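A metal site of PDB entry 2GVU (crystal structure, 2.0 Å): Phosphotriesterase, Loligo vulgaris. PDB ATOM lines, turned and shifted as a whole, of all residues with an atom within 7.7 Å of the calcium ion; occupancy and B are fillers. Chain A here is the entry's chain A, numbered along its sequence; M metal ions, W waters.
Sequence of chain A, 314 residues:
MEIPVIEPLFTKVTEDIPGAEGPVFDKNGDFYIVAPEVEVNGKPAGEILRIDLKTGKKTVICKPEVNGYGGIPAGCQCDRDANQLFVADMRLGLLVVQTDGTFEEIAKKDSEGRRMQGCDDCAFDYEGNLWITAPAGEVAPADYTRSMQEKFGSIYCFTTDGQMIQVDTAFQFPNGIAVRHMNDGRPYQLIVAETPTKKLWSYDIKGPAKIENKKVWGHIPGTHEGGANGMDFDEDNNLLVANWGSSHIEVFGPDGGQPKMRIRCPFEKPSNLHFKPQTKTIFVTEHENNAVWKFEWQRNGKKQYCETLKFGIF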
ATOM      1  N   GLY A  22      -6.502  -3.518  -1.468  1.00  0.00           N
ATOM      2  CA  GLY A  22      -6.300  -3.329  -0.035  1.00  0.00           C
ATOM      3  C   GLY A  22      -7.037  -4.179   0.992  1.00  0.00           C
ATOM      4  O   GLY A  22      -7.617  -3.626   1.932  1.00  0.00           O
ATOM      5  N   PRO A  23      -7.034  -5.508   0.858  1.00  0.00           N
ATOM      6  CA  PRO A  23      -7.746  -6.305   1.861  1.00  0.00           C
ATOM      7  C   PRO A  23      -7.090  -6.143   3.237  1.00  0.00           C
ATOM      8  O   PRO A  23      -5.869  -6.155   3.354  1.00  0.00           O
ATOM      9  CB  PRO A  23      -7.637  -7.722   1.324  1.00  0.00           C
ATOM     10  CG  PRO A  23      -6.303  -7.709   0.608  1.00  0.00           C
ATOM     11  CD  PRO A  23      -6.314  -6.375  -0.097  1.00  0.00           C
ATOM     12  N   VAL A  24      -7.909  -5.993   4.263  1.00  0.00           N
ATOM     13  CA  VAL A  24      -7.365  -5.805   5.599  1.00  0.00           C
ATOM     14  C   VAL A  24      -8.356  -6.196   6.700  1.00  0.00           C
ATOM     15  O   VAL A  24      -9.572  -6.175   6.487  1.00  0.00           O
ATOM     16  CB  VAL A  24      -6.949  -4.335   5.774  1.00  0.00           C
ATOM     17  CG1 VAL A  24      -8.181  -3.452   5.827  1.00  0.00           C
ATOM     18  CG2 VAL A  24      -6.096  -4.174   7.025  1.00  0.00           C
ATOM     19  N   PHE A  25      -7.829  -6.554   7.856  1.00  0.00           N
ATOM     20  CA  PHE A  25      -8.636  -6.922   9.024  1.00  0.00           C
ATOM     21  C   PHE A  25      -8.333  -5.918  10.124  1.00  0.00           C
ATOM     22  O   PHE A  25      -7.169  -5.565  10.324  1.00  0.00           O
ATOM     23  CB  PHE A  25      -8.280  -8.324   9.507  1.00  0.00           C
ATOM     24  CG  PHE A  25      -8.878  -9.431   8.688  1.00  0.00           C
ATOM     25  CD1 PHE A  25     -10.191  -9.837   8.905  1.00  0.00           C
ATOM     26  CD2 PHE A  25      -8.140 -10.050   7.680  1.00  0.00           C
ATOM     27  CE1 PHE A  25     -10.766 -10.857   8.146  1.00  0.00           C
ATOM     28  CE2 PHE A  25      -8.697 -11.071   6.906  1.00  0.00           C
ATOM     29  CZ  PHE A  25     -10.013 -11.471   7.147  1.00  0.00           C
ATOM     30  N   CYS A  76      -4.413  -0.579   2.518  1.00  0.00           N
ATOM     31  CA  CYS A  76      -4.734  -0.371   3.927  1.00  0.00           C
ATOM     32  C   CYS A  76      -3.832  -1.095   4.930  1.00  0.00           C
ATOM     33  O   CYS A  76      -3.210  -2.096   4.614  1.00  0.00           O
ATOM     34  CB  CYS A  76      -6.165  -0.835   4.210  1.00  0.00           C
ATOM     35  SG  CYS A  76      -7.397  -0.258   3.046  1.00  0.00           S
ATOM     36  N   GLN A  77      -3.833  -0.556   6.148  1.00  0.00           N
ATOM     37  CA  GLN A  77      -3.101  -1.126   7.268  1.00  0.00           C
ATOM     38  C   GLN A  77      -3.948  -0.847   8.509  1.00  0.00           C
ATOM     39  O   GLN A  77      -4.552   0.210   8.644  1.00  0.00           O
ATOM     40  CB  GLN A  77      -1.723  -0.485   7.442  1.00  0.00           C
ATOM     41  CG  GLN A  77      -0.616  -1.082   6.551  1.00  0.00           C
ATOM     42  CD  GLN A  77      -0.392  -2.567   6.787  1.00  0.00           C
ATOM     43  OE1 GLN A  77      -0.990  -3.414   6.126  1.00  0.00           O
ATOM     44  NE2 GLN A  77       0.455  -2.891   7.755  1.00  0.00           N
ATOM     45  N   ASP A 121       0.102   1.630  -1.397  1.00  0.00           N
ATOM     46  CA  ASP A 121       0.018   0.631  -0.329  1.00  0.00           C
ATOM     47  C   ASP A 121       0.904   1.067   0.829  1.00  0.00           C
ATOM     48  O   ASP A 121       1.700   1.994   0.694  1.00  0.00           O
ATOM     49  CB  ASP A 121       0.481  -0.740  -0.847  1.00  0.00           C
ATOM     50  CG  ASP A 121      -0.271  -1.913  -0.205  1.00  0.00           C
ATOM     51  OD1 ASP A 121      -0.857  -1.750   0.884  1.00  0.00           O
ATOM     52  OD2 ASP A 121      -0.256  -3.012  -0.791  1.00  0.00           O
ATOM     53  N   CYS A 122       0.766   0.403   1.971  1.00  0.00           N
ATOM     54  CA  CYS A 122       1.555   0.755   3.142  1.00  0.00           C
ATOM     55  C   CYS A 122       1.745  -0.455   4.050  1.00  0.00           C
ATOM     56  O   CYS A 122       1.031  -1.443   3.934  1.00  0.00           O
ATOM     57  CB  CYS A 122       0.861   1.886   3.918  1.00  0.00           C
ATOM     58  SG  CYS A 122      -0.886   1.572   4.258  1.00  0.00           S
ATOM     59  N   ILE A 177       4.512  -3.311  -0.586  1.00  0.00           N
ATOM     60  CA  ILE A 177       5.590  -2.999   0.341  1.00  0.00           C
ATOM     61  C   ILE A 177       5.396  -3.850   1.584  1.00  0.00           C
ATOM     62  O   ILE A 177       4.267  -4.086   2.026  1.00  0.00           O
ATOM     63  CB  ILE A 177       5.576  -1.489   0.678  1.00  0.00           C
ATOM     64  CG1 ILE A 177       6.751  -1.145   1.589  1.00  0.00           C
ATOM     65  CG2 ILE A 177       4.232  -1.111   1.301  1.00  0.00           C
ATOM     66  CD1 ILE A 177       6.991   0.357   1.721  1.00  0.00           C
ATOM     67  N   GLY A 230       0.487  -6.362  -4.661  1.00  0.00           N
ATOM     68  CA  GLY A 230       0.514  -6.472  -3.204  1.00  0.00           C
ATOM     69  C   GLY A 230       1.299  -7.641  -2.636  1.00  0.00           C
ATOM     70  O   GLY A 230       1.500  -8.647  -3.329  1.00  0.00           O
ATOM     71  N   MET A 231       1.710  -7.531  -1.374  1.00  0.00           N
ATOM     72  CA  MET A 231       2.490  -8.581  -0.719  1.00  0.00           C
ATOM     73  C   MET A 231       2.303  -8.641   0.806  1.00  0.00           C
ATOM     74  O   MET A 231       1.814  -7.696   1.426  1.00  0.00           O
ATOM     75  CB  MET A 231       3.980  -8.373  -1.003  1.00  0.00           C
ATOM     76  CG  MET A 231       4.547  -7.075  -0.401  1.00  0.00           C
ATOM     77  SD  MET A 231       6.297  -6.718  -0.794  1.00  0.00           S
ATOM     78  CE  MET A 231       6.303  -7.057  -2.502  1.00  0.00           C
ATOM     79  N   ASP A 232       2.731  -9.746   1.385  1.00  0.00           N
ATOM     80  CA  ASP A 232       2.678  -9.980   2.828  1.00  0.00           C
ATOM     81  C   ASP A 232       3.553 -11.182   3.151  1.00  0.00           C
ATOM     82  O   ASP A 232       3.761 -12.049   2.292  1.00  0.00           O
ATOM     83  CB  ASP A 232       1.240 -10.273   3.300  1.00  0.00           C
ATOM     84  CG  ASP A 232       0.450  -9.015   3.644  1.00  0.00           C
ATOM     85  OD1 ASP A 232       0.989  -8.149   4.379  1.00  0.00           O
ATOM     86  OD2 ASP A 232      -0.711  -8.894   3.201  1.00  0.00           O
ATOM     87  N   PHE A 233       4.052 -11.233   4.378  1.00  0.00           N
ATOM     88  CA  PHE A 233       4.897 -12.309   4.882  1.00  0.00           C
ATOM     89  C   PHE A 233       4.093 -13.350   5.659  1.00  0.00           C
ATOM     90  O   PHE A 233       3.074 -13.018   6.264  1.00  0.00           O
ATOM     91  CB  PHE A 233       5.955 -11.756   5.838  1.00  0.00           C
ATOM     92  CG  PHE A 233       7.150 -11.141   5.175  1.00  0.00           C
ATOM     93  CD1 PHE A 233       8.084 -11.928   4.530  1.00  0.00           C
ATOM     94  CD2 PHE A 233       7.343  -9.757   5.222  1.00  0.00           C
ATOM     95  CE1 PHE A 233       9.209 -11.353   3.937  1.00  0.00           C
ATOM     96  CE2 PHE A 233       8.470  -9.172   4.632  1.00  0.00           C
ATOM     97  CZ  PHE A 233       9.400  -9.978   3.983  1.00  0.00           C
ATOM     98  N   ASN A 272      -3.856  -7.963  -4.592  1.00  0.00           N
ATOM     99  CA  ASN A 272      -3.327  -7.829  -3.236  1.00  0.00           C
ATOM    100  C   ASN A 272      -3.820  -9.002  -2.402  1.00  0.00           C
ATOM    101  O   ASN A 272      -4.650  -9.784  -2.849  1.00  0.00           O
ATOM    102  CB  ASN A 272      -3.795  -6.515  -2.594  1.00  0.00           C
ATOM    103  CG  ASN A 272      -2.740  -5.886  -1.691  1.00  0.00           C
ATOM    104  OD1 ASN A 272      -1.974  -6.579  -1.018  1.00  0.00           O
ATOM    105  ND2 ASN A 272      -2.693  -4.566  -1.668  1.00  0.00           N
ATOM    106  N   LEU A 273      -3.310  -9.097  -1.179  1.00  0.00           N
ATOM    107  CA  LEU A 273      -3.688 -10.198  -0.322  1.00  0.00           C
ATOM    108  C   LEU A 273      -3.517  -9.843   1.154  1.00  0.00           C
ATOM    109  O   LEU A 273      -2.949  -8.803   1.492  1.00  0.00           O
ATOM    110  CB  LEU A 273      -2.872 -11.447  -0.692  1.00  0.00           C
ATOM    111  CG  LEU A 273      -1.358 -11.250  -0.857  1.00  0.00           C
ATOM    112  CD1 LEU A 273      -0.688 -11.265   0.498  1.00  0.00           C
ATOM    113  CD2 LEU A 273      -0.785 -12.362  -1.726  1.00  0.00           C
ATOM    114  N   HIS A 274      -4.008 -10.707   2.019  1.00  0.00           N
ATOM    115  CA  HIS A 274      -3.917 -10.467   3.440  1.00  0.00           C
ATOM    116  C   HIS A 274      -4.346 -11.720   4.182  1.00  0.00           C
ATOM    117  O   HIS A 274      -5.263 -12.409   3.741  1.00  0.00           O
ATOM    118  CB  HIS A 274      -4.825  -9.307   3.840  1.00  0.00           C
ATOM    119  CG  HIS A 274      -4.310  -8.504   4.991  1.00  0.00           C
ATOM    120  ND1 HIS A 274      -3.193  -7.699   4.902  1.00  0.00           N
ATOM    121  CD2 HIS A 274      -4.763  -8.381   6.260  1.00  0.00           C
ATOM    122  CE1 HIS A 274      -2.979  -7.118   6.067  1.00  0.00           C
ATOM    123  NE2 HIS A 274      -3.923  -7.518   6.908  1.00  0.00           N
ATOM    124  N   PHE A 275      -3.680 -11.999   5.294  1.00  0.00           N
ATOM    125  CA  PHE A 275      -3.994 -13.161   6.118  1.00  0.00           C
ATOM    126  C   PHE A 275      -5.070 -12.829   7.131  1.00  0.00           C
ATOM    127  O   PHE A 275      -5.125 -11.716   7.646  1.00  0.00           O
ATOM    128  CB  PHE A 275      -2.767 -13.615   6.912  1.00  0.00           C
ATOM    129  CG  PHE A 275      -1.774 -14.429   6.127  1.00  0.00           C
ATOM    130  CD1 PHE A 275      -0.781 -13.811   5.388  1.00  0.00           C
ATOM    131  CD2 PHE A 275      -1.818 -15.824   6.157  1.00  0.00           C
ATOM    132  CE1 PHE A 275       0.163 -14.555   4.678  1.00  0.00           C
ATOM    133  CE2 PHE A 275      -0.884 -16.578   5.457  1.00  0.00           C
ATOM    134  CZ  PHE A 275       0.099 -15.946   4.713  1.00  0.00           C
ATOM    135  N   PHE A 283      -6.824 -13.905   2.073  1.00  0.00           N
ATOM    136  CA  PHE A 283      -7.863 -13.326   1.267  1.00  0.00           C
ATOM    137  C   PHE A 283      -7.174 -12.598   0.121  1.00  0.00           C
ATOM    138  O   PHE A 283      -6.226 -11.838   0.340  1.00  0.00           O
ATOM    139  CB  PHE A 283      -8.721 -12.365   2.091  1.00  0.00           C
ATOM    140  CG  PHE A 283      -9.672 -13.066   3.021  1.00  0.00           C
ATOM    141  CD1 PHE A 283      -9.197 -13.722   4.150  1.00  0.00           C
ATOM    142  CD2 PHE A 283     -11.029 -13.122   2.737  1.00  0.00           C
ATOM    143  CE1 PHE A 283     -10.069 -14.422   4.986  1.00  0.00           C
ATOM    144  CE2 PHE A 283     -11.914 -13.818   3.567  1.00  0.00           C
ATOM    145  CZ  PHE A 283     -11.429 -14.475   4.693  1.00  0.00           C
ATOM    146  N   GLN A 304       0.486  -8.866  12.005  1.00  0.00           N
ATOM    147  CA  GLN A 304       0.507  -7.479  11.551  1.00  0.00           C
ATOM    148  C   GLN A 304       0.721  -6.644  12.808  1.00  0.00           C
ATOM    149  O   GLN A 304       0.545  -7.126  13.925  1.00  0.00           O
ATOM    150  CB  GLN A 304      -0.829  -7.103  10.902  1.00  0.00           C
ATOM    151  CG  GLN A 304      -1.080  -7.724   9.532  1.00  0.00           C
ATOM    152  CD  GLN A 304      -0.306  -7.017   8.435  1.00  0.00           C
ATOM    153  OE1 GLN A 304       0.654  -7.549   7.897  1.00  0.00           O
ATOM    154  NE2 GLN A 304      -0.732  -5.799   8.111  1.00  0.00           N
HETATM  155 CA    CA M   1      -1.998  -7.327   2.976  1.00  0.00          CA
HETATM  156  O   HOH W   1      -0.769  -5.946   4.385  1.00  0.00           O
HETATM  157  O   HOH W   2      -3.563  -5.895   2.228  1.00  0.00           O
HETATM  158  O   HOH W   3      -0.738  -6.692   1.213  1.00  0.00           O
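A ring nitrogen (ND1) of His 274 sits close to the backbone carbonyl oxygen of Pro 23, 3.5 Å away. The backbone NH (N) of Phe 283 sits at hydrogen-bond distance from the backbone carbonyl oxygen (O) of His 274, 2.7 Å away.
The calcium ion is bound by the side-chain carboxylate (OD2) of Asp 232. Water W2 binds the calcium ion (2.2 Å). The calcium ion is bound by water W3, 2.3 Å away. ND1 of His 274 is bound to the calcium ion (2.3 Å). O of Leu 273 binds the calcium ion (2.3 Å). Water W1 is bound to the calcium ion. The calcium ion has six donor atoms within binding distance.
Three residues have an atom within 4 Å of the calcium ion: Asp 232, Leu 273 and His 274.
Water W1 lies within hydrogen-bond range of OD1 of Asp 232 (2.8 Å) and OE1 of Gln 77 (3.1 Å). Water W3 bridges OD1 of Asn 272 and O of Met 231.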
